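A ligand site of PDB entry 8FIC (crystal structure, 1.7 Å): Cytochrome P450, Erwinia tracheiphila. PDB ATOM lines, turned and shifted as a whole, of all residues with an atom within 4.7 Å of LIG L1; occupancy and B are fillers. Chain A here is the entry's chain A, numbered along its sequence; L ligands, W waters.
FE1 of LIG L1 is bound by SG of Cys 388 (2.3 Å).
O2 of LIG L1 lies within hydrogen-bond range of OG of Ser 316, 2.5 Å away.
O4 of LIG L1 sits at hydrogen-bond distance from NE2 of His 114.
O4 of LIG L1 is in salt-bridge range of NH1 of Arg 118 (2.7 Å).
NH2 of Arg 320 lies within salt-bridge range of O1 of LIG L1 (2.7 Å).
ND1 of His 386 lies within hydrogen-bond range of O3 of LIG L1 (2.8 Å).
OG of Ser 316 lies within hydrogen-bond range of O1 of LG2 L2, 2.8 Å away.
The backbone carbonyl oxygen (O) of Phe 381 sits at hydrogen-bond distance from the backbone NH (N) of Cys 388, at 3.0 Å.
The side-chain sulfur of Cys 388 lies close to the backbone NH of Gly 390 (3.2 Å).
The side-chain hydroxyl (OG) of Ser 316 is in hydrogen-bond range of the backbone NH (N) of Ile 318 (3.1 Å).
A ring nitrogen (NE2) of His 114 lies close to the backbone carbonyl oxygen of Ile 385 (3.2 Å).
NH1 of Arg 118 sits at hydrogen-bond distance from O of Ile 385 (3.4 Å).
O of Phe 387 lies within hydrogen-bond range of NH1 of Arg 118.
A ring nitrogen (NE2) of His 386 sits close to the backbone carbonyl oxygen (O) of Ala 107 (3.2 Å).
OG of Ser 380 sits at hydrogen-bond distance from O of Leu 307.
An oxygen (O4) of LIG L1 sits close to the backbone carbonyl oxygen of Ile 385 (3.4 Å).
Leu 106 touches LIG L1 (CG to O3, 3.7 Å).
Ala 107 touches LIG L1 (CA to O3, 3.5 Å).
Phe 125 touches LIG L1.
CG2 of Ile 263 touches C26 of LIG L1, 3.6 Å away.
O of Gly 266 touches C21 of LIG L1 (3.2 Å).
Gly 267 touches LIG L1.
OG1 of Thr 270 touches C15 of LIG L1, at 3.3 Å.
Thr 271 touches LIG L1 (OG1 to C24, 3.7 Å).
CG of Met 274 touches C19 of LIG L1, at 3.2 Å.
Pro 312 touches LIG L1 (CG to C17, 3.2 Å).
Ile 318 touches LIG L1.
CD1 of Leu 343 touches C9 of LIG L1, 3.6 Å away.
Ser 380 touches LIG L1.
Phe 381 touches LIG L1.
Gly 382 touches LIG L1 (N to C9, 3.8 Å).
O of Phe 387 touches C33 of LIG L1, 3.97 Å away.
N of Leu 389 touches N4 of LIG L1 (3.7 Å).
Gly 390 touches LIG L1.
CD2 of Leu 393 touches C24 of LIG L1 (3.9 Å).
CB of Ala 394 touches C18 of LIG L1 (3.7 Å).
Hydrophobic or aromatic side chains that line LIG L1: Leu 106, Ala 107, His 114, Phe 125, Ile 263, Met 274, Pro 312, Ile 318, Leu 343, Phe 381, His 386, Leu 389, Leu 393 and Ala 394.
Of the 31 residues printed, 27 come within 4 Å of LIG L1.
Water W2 bridges an oxygen (O1) of LIG L1 (2.6 Å) and the backbone carbonyl oxygen of His 386 (3.1 Å).
Water W1 bridges the side-chain hydroxyl (OG1) of Thr 270 and the backbone carbonyl oxygen (O) of Gly 266.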
ATOM      1  N   LEU A  71      22.897 -14.323  -8.619  1.00  0.00           N
ATOM      2  CA  LEU A  71      22.582 -14.995  -9.873  1.00  0.00           C
ATOM      3  C   LEU A  71      21.080 -15.206 -10.009  1.00  0.00           C
ATOM      4  O   LEU A  71      20.483 -14.897 -11.037  1.00  0.00           O
ATOM      5  CB  LEU A  71      23.321 -16.324  -9.954  1.00  0.00           C
ATOM      6  CG  LEU A  71      24.839 -16.273 -10.041  1.00  0.00           C
ATOM      7  CD1 LEU A  71      25.425 -17.668  -9.808  1.00  0.00           C
ATOM      8  CD2 LEU A  71      25.271 -15.735 -11.400  1.00  0.00           C
ATOM      9  N   LEU A 106      23.064 -11.976 -25.359  1.00  0.00           N
ATOM     10  CA  LEU A 106      21.904 -12.259 -24.530  1.00  0.00           C
ATOM     11  C   LEU A 106      22.256 -12.316 -23.057  1.00  0.00           C
ATOM     12  O   LEU A 106      21.362 -12.192 -22.207  1.00  0.00           O
ATOM     13  CB  LEU A 106      21.240 -13.563 -24.969  1.00  0.00           C
ATOM     14  CG  LEU A 106      21.847 -14.885 -24.498  1.00  0.00           C
ATOM     15  CD1 LEU A 106      20.890 -16.038 -24.774  1.00  0.00           C
ATOM     16  CD2 LEU A 106      23.199 -15.158 -25.163  1.00  0.00           C
ATOM     17  N   ALA A 107      23.529 -12.516 -22.709  1.00  0.00           N
ATOM     18  CA  ALA A 107      23.930 -12.533 -21.307  1.00  0.00           C
ATOM     19  C   ALA A 107      23.800 -11.167 -20.649  1.00  0.00           C
ATOM     20  O   ALA A 107      23.826 -11.086 -19.415  1.00  0.00           O
ATOM     21  CB  ALA A 107      25.370 -13.036 -21.167  1.00  0.00           C
ATOM     22  N   HIS A 114      15.867 -11.286 -23.554  1.00  0.00           N
ATOM     23  CA  HIS A 114      16.648 -12.489 -23.280  1.00  0.00           C
ATOM     24  C   HIS A 114      15.912 -13.738 -23.715  1.00  0.00           C
ATOM     25  O   HIS A 114      16.499 -14.649 -24.308  1.00  0.00           O
ATOM     26  CB  HIS A 114      16.987 -12.580 -21.795  1.00  0.00           C
ATOM     27  CG  HIS A 114      17.625 -13.867 -21.409  1.00  0.00           C
ATOM     28  ND1 HIS A 114      16.926 -14.938 -20.907  1.00  0.00           N
ATOM     29  CD2 HIS A 114      18.920 -14.266 -21.490  1.00  0.00           C
ATOM     30  CE1 HIS A 114      17.755 -15.938 -20.679  1.00  0.00           C
ATOM     31  NE2 HIS A 114      18.965 -15.564 -21.031  1.00  0.00           N
ATOM     32  N   ARG A 118      17.433 -16.343 -26.414  1.00  0.00           N
ATOM     33  CA  ARG A 118      17.743 -17.703 -25.998  1.00  0.00           C
ATOM     34  C   ARG A 118      16.892 -18.706 -26.764  1.00  0.00           C
ATOM     35  O   ARG A 118      17.362 -19.807 -27.100  1.00  0.00           O
ATOM     36  CB  ARG A 118      17.533 -17.861 -24.488  1.00  0.00           C
ATOM     37  CG  ARG A 118      17.904 -19.241 -23.979  1.00  0.00           C
ATOM     38  CD  ARG A 118      18.494 -19.201 -22.586  1.00  0.00           C
ATOM     39  NE  ARG A 118      18.882 -20.534 -22.130  1.00  0.00           N
ATOM     40  CZ  ARG A 118      19.803 -20.776 -21.202  1.00  0.00           C
ATOM     41  NH1 ARG A 118      20.452 -19.768 -20.631  1.00  0.00           N
ATOM     42  NH2 ARG A 118      20.073 -22.025 -20.845  1.00  0.00           N
ATOM     43  N   ILE A 121      18.477 -20.115 -30.011  1.00  0.00           N
ATOM     44  CA  ILE A 121      19.658 -20.967 -29.990  1.00  0.00           C
ATOM     45  C   ILE A 121      19.497 -22.192 -29.109  1.00  0.00           C
ATOM     46  O   ILE A 121      20.400 -23.053 -29.106  1.00  0.00           O
ATOM     47  CB  ILE A 121      20.903 -20.166 -29.543  1.00  0.00           C
ATOM     48  CG1 ILE A 121      20.727 -19.643 -28.109  1.00  0.00           C
ATOM     49  CG2 ILE A 121      21.146 -18.999 -30.495  1.00  0.00           C
ATOM     50  CD1 ILE A 121      21.944 -18.907 -27.564  1.00  0.00           C
ATOM     51  N   PHE A 125      21.218 -27.128 -28.261  1.00  0.00           N
ATOM     52  CA  PHE A 125      21.937 -27.491 -27.041  1.00  0.00           C
ATOM     53  C   PHE A 125      21.112 -28.379 -26.119  1.00  0.00           C
ATOM     54  O   PHE A 125      21.550 -28.664 -25.004  1.00  0.00           O
ATOM     55  CB  PHE A 125      22.376 -26.230 -26.312  1.00  0.00           C
ATOM     56  CG  PHE A 125      23.408 -25.427 -27.063  1.00  0.00           C
ATOM     57  CD1 PHE A 125      24.753 -25.687 -26.905  1.00  0.00           C
ATOM     58  CD2 PHE A 125      23.010 -24.449 -27.955  1.00  0.00           C
ATOM     59  CE1 PHE A 125      25.702 -24.957 -27.623  1.00  0.00           C
ATOM     60  CE2 PHE A 125      23.936 -23.716 -28.665  1.00  0.00           C
ATOM     61  CZ  PHE A 125      25.285 -23.971 -28.495  1.00  0.00           C
ATOM     62  N   PHE A 173      32.251 -28.338 -31.295  1.00  0.00           N
ATOM     63  CA  PHE A 173      31.561 -27.052 -31.420  1.00  0.00           C
ATOM     64  C   PHE A 173      31.453 -26.632 -32.884  1.00  0.00           C
ATOM     65  O   PHE A 173      30.398 -26.157 -33.320  1.00  0.00           O
ATOM     66  CB  PHE A 173      32.283 -25.986 -30.607  1.00  0.00           C
ATOM     67  CG  PHE A 173      31.744 -24.611 -30.849  1.00  0.00           C
ATOM     68  CD1 PHE A 173      30.584 -24.205 -30.220  1.00  0.00           C
ATOM     69  CD2 PHE A 173      32.375 -23.739 -31.712  1.00  0.00           C
ATOM     70  CE1 PHE A 173      30.077 -22.945 -30.438  1.00  0.00           C
ATOM     71  CE2 PHE A 173      31.869 -22.487 -31.935  1.00  0.00           C
ATOM     72  CZ  PHE A 173      30.715 -22.084 -31.299  1.00  0.00           C
ATOM     73  N   ILE A 263      28.872 -16.755 -28.867  1.00  0.00           N
ATOM     74  CA  ILE A 263      28.834 -18.215 -28.796  1.00  0.00           C
ATOM     75  C   ILE A 263      30.198 -18.805 -29.148  1.00  0.00           C
ATOM     76  O   ILE A 263      30.628 -19.794 -28.561  1.00  0.00           O
ATOM     77  CB  ILE A 263      27.704 -18.762 -29.685  1.00  0.00           C
ATOM     78  CG1 ILE A 263      26.353 -18.334 -29.099  1.00  0.00           C
ATOM     79  CG2 ILE A 263      27.801 -20.287 -29.795  1.00  0.00           C
ATOM     80  CD1 ILE A 263      25.162 -18.692 -29.968  1.00  0.00           C
ATOM     81  N   GLY A 266      32.298 -18.631 -26.093  1.00  0.00           N
ATOM     82  CA  GLY A 266      31.934 -19.613 -25.095  1.00  0.00           C
ATOM     83  C   GLY A 266      32.062 -21.049 -25.538  1.00  0.00           C
ATOM     84  O   GLY A 266      31.959 -21.960 -24.709  1.00  0.00           O
ATOM     85  N   GLY A 267      32.334 -21.276 -26.823  1.00  0.00           N
ATOM     86  CA  GLY A 267      32.076 -22.564 -27.446  1.00  0.00           C
ATOM     87  C   GLY A 267      33.061 -23.680 -27.110  1.00  0.00           C
ATOM     88  O   GLY A 267      32.686 -24.865 -27.254  1.00  0.00           O
ATOM     89  N   THR A 270      36.398 -22.873 -22.288  1.00  0.00           N
ATOM     90  CA  THR A 270      36.102 -23.331 -20.937  1.00  0.00           C
ATOM     91  C   THR A 270      35.963 -24.847 -20.867  1.00  0.00           C
ATOM     92  O   THR A 270      36.279 -25.456 -19.845  1.00  0.00           O
ATOM     93  CB  THR A 270      34.830 -22.682 -20.416  1.00  0.00           C
ATOM     94  OG1 THR A 270      33.844 -22.674 -21.452  1.00  0.00           O
ATOM     95  CG2 THR A 270      35.101 -21.268 -19.939  1.00  0.00           C
ATOM     96  N   THR A 271      35.450 -25.471 -21.932  1.00  0.00           N
ATOM     97  CA  THR A 271      35.346 -26.924 -21.954  1.00  0.00           C
ATOM     98  C   THR A 271      36.731 -27.572 -21.966  1.00  0.00           C
ATOM     99  O   THR A 271      36.988 -28.517 -21.214  1.00  0.00           O
ATOM    100  CB  THR A 271      34.516 -27.377 -23.153  1.00  0.00           C
ATOM    101  OG1 THR A 271      33.216 -26.774 -23.097  1.00  0.00           O
ATOM    102  CG2 THR A 271      34.352 -28.888 -23.158  1.00  0.00           C
ATOM    103  N   MET A 274      38.154 -27.511 -18.615  1.00  0.00           N
ATOM    104  CA  MET A 274      37.632 -28.539 -17.732  1.00  0.00           C
ATOM    105  C   MET A 274      38.222 -29.901 -18.045  1.00  0.00           C
ATOM    106  O   MET A 274      38.417 -30.712 -17.123  1.00  0.00           O
ATOM    107  CB  MET A 274      36.109 -28.594 -17.798  1.00  0.00           C
ATOM    108  CG  MET A 274      35.429 -27.388 -17.197  1.00  0.00           C
ATOM    109  SD  MET A 274      36.275 -26.704 -15.745  1.00  0.00           S
ATOM    110  CE  MET A 274      36.311 -28.088 -14.614  1.00  0.00           C
ATOM    111  N   LEU A 307      34.013 -30.016 -11.848  1.00  0.00           N
ATOM    112  CA  LEU A 307      33.475 -28.688 -12.111  1.00  0.00           C
ATOM    113  C   LEU A 307      33.422 -27.840 -10.842  1.00  0.00           C
ATOM    114  O   LEU A 307      33.630 -26.625 -10.901  1.00  0.00           O
ATOM    115  CB  LEU A 307      32.076 -28.818 -12.721  1.00  0.00           C
ATOM    116  CG  LEU A 307      32.052 -29.260 -14.178  1.00  0.00           C
ATOM    117  CD1 LEU A 307      30.685 -29.799 -14.589  1.00  0.00           C
ATOM    118  CD2 LEU A 307      32.439 -28.095 -15.079  1.00  0.00           C
ATOM    119  N   PRO A 312      36.297 -22.969 -14.446  1.00  0.00           N
ATOM    120  CA  PRO A 312      37.240 -22.411 -15.429  1.00  0.00           C
ATOM    121  C   PRO A 312      37.145 -20.908 -15.558  1.00  0.00           C
ATOM    122  O   PRO A 312      38.094 -20.279 -16.047  1.00  0.00           O
ATOM    123  CB  PRO A 312      36.851 -23.111 -16.740  1.00  0.00           C
ATOM    124  CG  PRO A 312      35.459 -23.481 -16.574  1.00  0.00           C
ATOM    125  CD  PRO A 312      35.153 -23.635 -15.102  1.00  0.00           C
ATOM    126  N   SER A 316      32.573 -14.143 -13.595  1.00  0.00           N
ATOM    127  CA  SER A 316      32.049 -13.934 -14.946  1.00  0.00           C
ATOM    128  C   SER A 316      32.303 -12.512 -15.432  1.00  0.00           C
ATOM    129  O   SER A 316      32.226 -11.549 -14.677  1.00  0.00           O
ATOM    130  CB  SER A 316      30.542 -14.228 -14.984  1.00  0.00           C
ATOM    131  OG  SER A 316      29.988 -13.829 -16.228  1.00  0.00           O
ATOM    132  N   ILE A 318      30.348 -10.929 -17.225  1.00  0.00           N
ATOM    133  CA  ILE A 318      29.055 -10.281 -17.398  1.00  0.00           C
ATOM    134  C   ILE A 318      28.770  -9.399 -16.185  1.00  0.00           C
ATOM    135  O   ILE A 318      28.684  -9.903 -15.061  1.00  0.00           O
ATOM    136  CB  ILE A 318      27.928 -11.305 -17.591  1.00  0.00           C
ATOM    137  CG1 ILE A 318      28.221 -12.229 -18.772  1.00  0.00           C
ATOM    138  CG2 ILE A 318      26.595 -10.594 -17.786  1.00  0.00           C
ATOM    139  CD1 ILE A 318      28.533 -11.516 -20.089  1.00  0.00           C
ATOM    140  N   ARG A 320      26.554  -7.245 -13.541  1.00  0.00           N
ATOM    141  CA  ARG A 320      25.217  -7.233 -12.969  1.00  0.00           C
ATOM    142  C   ARG A 320      25.068  -5.905 -12.252  1.00  0.00           C
ATOM    143  O   ARG A 320      25.811  -5.628 -11.301  1.00  0.00           O
ATOM    144  CB  ARG A 320      25.013  -8.409 -12.028  1.00  0.00           C
ATOM    145  CG  ARG A 320      24.833  -9.715 -12.772  1.00  0.00           C
ATOM    146  CD  ARG A 320      24.797 -10.926 -11.874  1.00  0.00           C
ATOM    147  NE  ARG A 320      24.242 -12.052 -12.611  1.00  0.00           N
ATOM    148  CZ  ARG A 320      24.915 -12.759 -13.512  1.00  0.00           C
ATOM    149  NH1 ARG A 320      26.180 -12.472 -13.780  1.00  0.00           N
ATOM    150  NH2 ARG A 320      24.311 -13.747 -14.160  1.00  0.00           N
ATOM    151  N   LEU A 343      32.507 -17.092  -8.676  1.00  0.00           N
ATOM    152  CA  LEU A 343      31.982 -18.452  -8.739  1.00  0.00           C
ATOM    153  C   LEU A 343      32.941 -19.466  -8.109  1.00  0.00           C
ATOM    154  O   LEU A 343      32.505 -20.361  -7.379  1.00  0.00           O
ATOM    155  CB  LEU A 343      31.736 -18.828 -10.205  1.00  0.00           C
ATOM    156  CG  LEU A 343      30.913 -17.834 -11.011  1.00  0.00           C
ATOM    157  CD1 LEU A 343      30.963 -18.201 -12.491  1.00  0.00           C
ATOM    158  CD2 LEU A 343      29.483 -17.803 -10.501  1.00  0.00           C
ATOM    159  N   SER A 380      29.807 -23.202 -11.243  1.00  0.00           N
ATOM    160  CA  SER A 380      30.686 -23.009 -12.389  1.00  0.00           C
ATOM    161  C   SER A 380      29.932 -22.699 -13.670  1.00  0.00           C
ATOM    162  O   SER A 380      30.524 -22.111 -14.587  1.00  0.00           O
ATOM    163  CB  SER A 380      31.545 -24.259 -12.563  1.00  0.00           C
ATOM    164  OG  SER A 380      32.133 -24.619 -11.333  1.00  0.00           O
ATOM    165  N   PHE A 381      28.656 -23.072 -13.756  1.00  0.00           N
ATOM    166  CA  PHE A 381      27.805 -22.782 -14.898  1.00  0.00           C
ATOM    167  C   PHE A 381      26.865 -21.605 -14.651  1.00  0.00           C
ATOM    168  O   PHE A 381      25.977 -21.355 -15.464  1.00  0.00           O
ATOM    169  CB  PHE A 381      26.953 -23.996 -15.254  1.00  0.00           C
ATOM    170  CG  PHE A 381      27.702 -25.124 -15.902  1.00  0.00           C
ATOM    171  CD1 PHE A 381      28.521 -24.905 -16.995  1.00  0.00           C
ATOM    172  CD2 PHE A 381      27.573 -26.415 -15.434  1.00  0.00           C
ATOM    173  CE1 PHE A 381      29.197 -25.956 -17.601  1.00  0.00           C
ATOM    174  CE2 PHE A 381      28.249 -27.473 -16.028  1.00  0.00           C
ATOM    175  CZ  PHE A 381      29.057 -27.234 -17.118  1.00  0.00           C
ATOM    176  N   GLY A 382      27.029 -20.897 -13.528  1.00  0.00           N
ATOM    177  CA  GLY A 382      26.076 -19.870 -13.174  1.00  0.00           C
ATOM    178  C   GLY A 382      24.784 -20.456 -12.635  1.00  0.00           C
ATOM    179  O   GLY A 382      24.718 -21.597 -12.178  1.00  0.00           O
ATOM    180  N   ILE A 385      18.593 -16.981 -14.923  1.00  0.00           N
ATOM    181  CA  ILE A 385      18.197 -16.828 -16.315  1.00  0.00           C
ATOM    182  C   ILE A 385      19.385 -17.035 -17.244  1.00  0.00           C
ATOM    183  O   ILE A 385      19.199 -17.455 -18.400  1.00  0.00           O
ATOM    184  CB  ILE A 385      17.528 -15.473 -16.587  1.00  0.00           C
ATOM    185  CG1 ILE A 385      18.475 -14.316 -16.301  1.00  0.00           C
ATOM    186  CG2 ILE A 385      16.224 -15.338 -15.794  1.00  0.00           C
ATOM    187  CD1 ILE A 385      17.930 -12.968 -16.776  1.00  0.00           C
ATOM    188  N   HIS A 386      20.601 -16.739 -16.794  1.00  0.00           N
ATOM    189  CA  HIS A 386      21.778 -16.896 -17.634  1.00  0.00           C
ATOM    190  C   HIS A 386      22.504 -18.214 -17.385  1.00  0.00           C
ATOM    191  O   HIS A 386      23.694 -18.334 -17.710  1.00  0.00           O
ATOM    192  CB  HIS A 386      22.739 -15.721 -17.453  1.00  0.00           C
ATOM    193  CG  HIS A 386      22.129 -14.384 -17.773  1.00  0.00           C
ATOM    194  ND1 HIS A 386      21.629 -14.078 -19.021  1.00  0.00           N
ATOM    195  CD2 HIS A 386      21.927 -13.289 -17.004  1.00  0.00           C
ATOM    196  CE1 HIS A 386      21.148 -12.847 -19.005  1.00  0.00           C
ATOM    197  NE2 HIS A 386      21.316 -12.342 -17.799  1.00  0.00           N
ATOM    198  N   PHE A 387      21.824 -19.209 -16.827  1.00  0.00           N
ATOM    199  CA  PHE A 387      22.463 -20.503 -16.645  1.00  0.00           C
ATOM    200  C   PHE A 387      23.031 -21.022 -17.954  1.00  0.00           C
ATOM    201  O   PHE A 387      22.379 -20.960 -19.006  1.00  0.00           O
ATOM    202  CB  PHE A 387      21.484 -21.529 -16.077  1.00  0.00           C
ATOM    203  CG  PHE A 387      22.123 -22.870 -15.858  1.00  0.00           C
ATOM    204  CD1 PHE A 387      22.906 -23.099 -14.741  1.00  0.00           C
ATOM    205  CD2 PHE A 387      21.989 -23.878 -16.806  1.00  0.00           C
ATOM    206  CE1 PHE A 387      23.511 -24.309 -14.534  1.00  0.00           C
ATOM    207  CE2 PHE A 387      22.597 -25.105 -16.610  1.00  0.00           C
ATOM    208  CZ  PHE A 387      23.369 -25.322 -15.478  1.00  0.00           C
ATOM    209  N   CYS A 388      24.234 -21.583 -17.876  1.00  0.00           N
ATOM    210  CA  CYS A 388      25.004 -21.960 -19.058  1.00  0.00           C
ATOM    211  C   CYS A 388      24.193 -22.763 -20.064  1.00  0.00           C
ATOM    212  O   CYS A 388      23.687 -23.840 -19.743  1.00  0.00           O
ATOM    213  CB  CYS A 388      26.232 -22.773 -18.651  1.00  0.00           C
ATOM    214  SG  CYS A 388      27.187 -23.315 -20.087  1.00  0.00           S
ATOM    215  N   LEU A 389      24.152 -22.264 -21.300  1.00  0.00           N
ATOM    216  CA  LEU A 389      23.477 -22.972 -22.379  1.00  0.00           C
ATOM    217  C   LEU A 389      24.220 -24.239 -22.779  1.00  0.00           C
ATOM    218  O   LEU A 389      23.605 -25.209 -23.225  1.00  0.00           O
ATOM    219  CB  LEU A 389      23.337 -22.044 -23.574  1.00  0.00           C
ATOM    220  CG  LEU A 389      22.569 -22.586 -24.782  1.00  0.00           C
ATOM    221  CD1 LEU A 389      21.088 -22.717 -24.434  1.00  0.00           C
ATOM    222  CD2 LEU A 389      22.776 -21.672 -25.976  1.00  0.00           C
ATOM    223  N   GLY A 390      25.544 -24.251 -22.628  1.00  0.00           N
ATOM    224  CA  GLY A 390      26.340 -25.362 -23.112  1.00  0.00           C
ATOM    225  C   GLY A 390      26.666 -26.409 -22.069  1.00  0.00           C
ATOM    226  O   GLY A 390      27.535 -27.254 -22.282  1.00  0.00           O
ATOM    227  N   LEU A 393      26.420 -29.939 -23.274  1.00  0.00           N
ATOM    228  CA  LEU A 393      27.462 -30.174 -24.265  1.00  0.00           C
ATOM    229  C   LEU A 393      28.794 -30.433 -23.583  1.00  0.00           C
ATOM    230  O   LEU A 393      29.523 -31.369 -23.947  1.00  0.00           O
ATOM    231  CB  LEU A 393      27.557 -28.981 -25.211  1.00  0.00           C
ATOM    232  CG  LEU A 393      28.671 -29.016 -26.256  1.00  0.00           C
ATOM    233  CD1 LEU A 393      28.594 -30.274 -27.104  1.00  0.00           C
ATOM    234  CD2 LEU A 393      28.612 -27.771 -27.124  1.00  0.00           C
ATOM    235  N   ALA A 394      29.147 -29.614 -22.601  1.00  0.00           N
ATOM    236  CA  ALA A 394      30.416 -29.791 -21.898  1.00  0.00           C
ATOM    237  C   ALA A 394      30.421 -31.097 -21.105  1.00  0.00           C
ATOM    238  O   ALA A 394      31.372 -31.886 -21.187  1.00  0.00           O
ATOM    239  CB  ALA A 394      30.686 -28.603 -20.987  1.00  0.00           C
HETATM  240  C1  LIG L   1      26.527 -18.879 -19.689  1.00  0.00           C
HETATM  241  C2  LIG L   1      30.397 -21.198 -17.879  1.00  0.00           C
HETATM  242  C3  LIG L   1      30.553 -24.043 -21.780  1.00  0.00           C
HETATM  243  C4  LIG L   1      27.469 -21.009 -23.963  1.00  0.00           C
HETATM  244  C5  LIG L   1      27.539 -19.261 -18.832  1.00  0.00           C
HETATM  245  C6  LIG L   1      27.831 -18.711 -17.522  1.00  0.00           C
HETATM  246  C7  LIG L   1      28.900 -19.362 -17.043  1.00  0.00           C
HETATM  247  C8  LIG L   1      29.327 -20.331 -18.025  1.00  0.00           C
HETATM  248  C9  LIG L   1      29.573 -19.135 -15.678  1.00  0.00           C
HETATM  249  C10 LIG L   1      27.016 -17.600 -16.807  1.00  0.00           C
HETATM  250  C11 LIG L   1      27.651 -16.233 -16.956  1.00  0.00           C
HETATM  251  C12 LIG L   1      26.964 -15.250 -16.026  1.00  0.00           C
HETATM  252  O1  LIG L   1      25.842 -15.555 -15.542  1.00  0.00           O
HETATM  253  O2  LIG L   1      27.550 -14.157 -15.774  1.00  0.00           O
HETATM  254  C13 LIG L   1      30.705 -22.238 -18.723  1.00  0.00           C
HETATM  255  C14 LIG L   1      31.570 -23.371 -18.440  1.00  0.00           C
HETATM  256  C15 LIG L   1      31.616 -24.156 -19.521  1.00  0.00           C
HETATM  257  C16 LIG L   1      30.773 -23.546 -20.524  1.00  0.00           C
HETATM  258  C17 LIG L   1      32.308 -23.612 -17.101  1.00  0.00           C
HETATM  259  C18 LIG L   1      32.370 -25.491 -19.746  1.00  0.00           C
HETATM  260  C19 LIG L   1      32.822 -26.245 -18.754  1.00  0.00           C
HETATM  261  C20 LIG L   1      29.749 -23.466 -22.733  1.00  0.00           C
HETATM  262  C21 LIG L   1      29.583 -23.932 -24.082  1.00  0.00           C
HETATM  263  C22 LIG L   1      28.747 -23.103 -24.717  1.00  0.00           C
HETATM  264  C23 LIG L   1      28.332 -22.078 -23.766  1.00  0.00           C
HETATM  265  C24 LIG L   1      30.286 -25.180 -24.666  1.00  0.00           C
HETATM  266  C25 LIG L   1      28.332 -23.304 -26.196  1.00  0.00           C
HETATM  267  C26 LIG L   1      27.612 -22.419 -26.887  1.00  0.00           C
HETATM  268  C27 LIG L   1      26.937 -20.187 -22.988  1.00  0.00           C
HETATM  269  C28 LIG L   1      25.937 -19.158 -23.203  1.00  0.00           C
HETATM  270  C29 LIG L   1      25.663 -18.567 -22.035  1.00  0.00           C
HETATM  271  C30 LIG L   1      26.479 -19.196 -21.029  1.00  0.00           C
HETATM  272  C31 LIG L   1      25.298 -18.813 -24.562  1.00  0.00           C
HETATM  273  C32 LIG L   1      24.656 -17.415 -21.808  1.00  0.00           C
HETATM  274  C33 LIG L   1      23.285 -17.988 -21.474  1.00  0.00           C
HETATM  275  C34 LIG L   1      22.254 -16.902 -21.224  1.00  0.00           C
HETATM  276  O3  LIG L   1      22.633 -15.726 -21.003  1.00  0.00           O
HETATM  277  O4  LIG L   1      21.033 -17.230 -21.227  1.00  0.00           O
HETATM  278  N1  LIG L   1      28.474 -20.234 -19.104  1.00  0.00           N
HETATM  279  N2  LIG L   1      30.242 -22.381 -20.020  1.00  0.00           N
HETATM  280  N3  LIG L   1      28.970 -22.336 -22.570  1.00  0.00           N
HETATM  281  N4  LIG L   1      27.249 -20.179 -21.636  1.00  0.00           N
HETATM  282 FE1  LIG L   1      28.530 -21.506 -20.751  1.00  0.00          FE
HETATM  283  C1  LG2 L   2      29.300 -16.260 -22.892  1.00  0.00           C
HETATM  284  C2  LG2 L   2      29.493 -13.694 -24.158  1.00  0.00           C
HETATM  285  C3  LG2 L   2      28.350 -15.103 -22.516  1.00  0.00           C
HETATM  286  C4  LG2 L   2      27.180 -15.437 -25.859  1.00  0.00           C
HETATM  287  C5  LG2 L   2      31.948 -15.718 -18.511  1.00  0.00           C
HETATM  288  C6  LG2 L   2      33.058 -15.370 -22.142  1.00  0.00           C
HETATM  289  C7  LG2 L   2      33.974 -15.333 -20.909  1.00  0.00           C
HETATM  290  C8  LG2 L   2      33.804 -16.555 -20.019  1.00  0.00           C
HETATM  291  C9  LG2 L   2      32.340 -16.756 -19.588  1.00  0.00           C
HETATM  292  C10 LG2 L   2      31.473 -16.790 -20.865  1.00  0.00           C
HETATM  293  C11 LG2 L   2      29.990 -17.105 -20.605  1.00  0.00           C
HETATM  294  C12 LG2 L   2      29.245 -17.386 -21.884  1.00  0.00           C
HETATM  295  C13 LG2 L   2      30.739 -15.772 -23.081  1.00  0.00           C
HETATM  296  C14 LG2 L   2      30.758 -14.553 -24.018  1.00  0.00           C
HETATM  297  C15 LG2 L   2      28.189 -14.381 -23.849  1.00  0.00           C
HETATM  298  C16 LG2 L   2      27.928 -15.519 -24.762  1.00  0.00           C
HETATM  299  C17 LG2 L   2      28.717 -16.697 -24.271  1.00  0.00           C
HETATM  300  C18 LG2 L   2      32.259 -18.077 -18.836  1.00  0.00           C
HETATM  301  C19 LG2 L   2      31.093 -14.250 -21.042  1.00  0.00           C
HETATM  302  C20 LG2 L   2      31.567 -15.520 -21.764  1.00  0.00           C
HETATM  303  O1  LG2 L   2      30.745 -15.678 -18.136  1.00  0.00           O
HETATM  304  O2  LG2 L   2      32.839 -14.970 -18.057  1.00  0.00           O
HETATM  305  O   HOH W   1      32.113 -20.749 -22.044  1.00  0.00           O
HETATM  306  O   HOH W   2      24.278 -17.553 -14.795  1.00  0.00           O
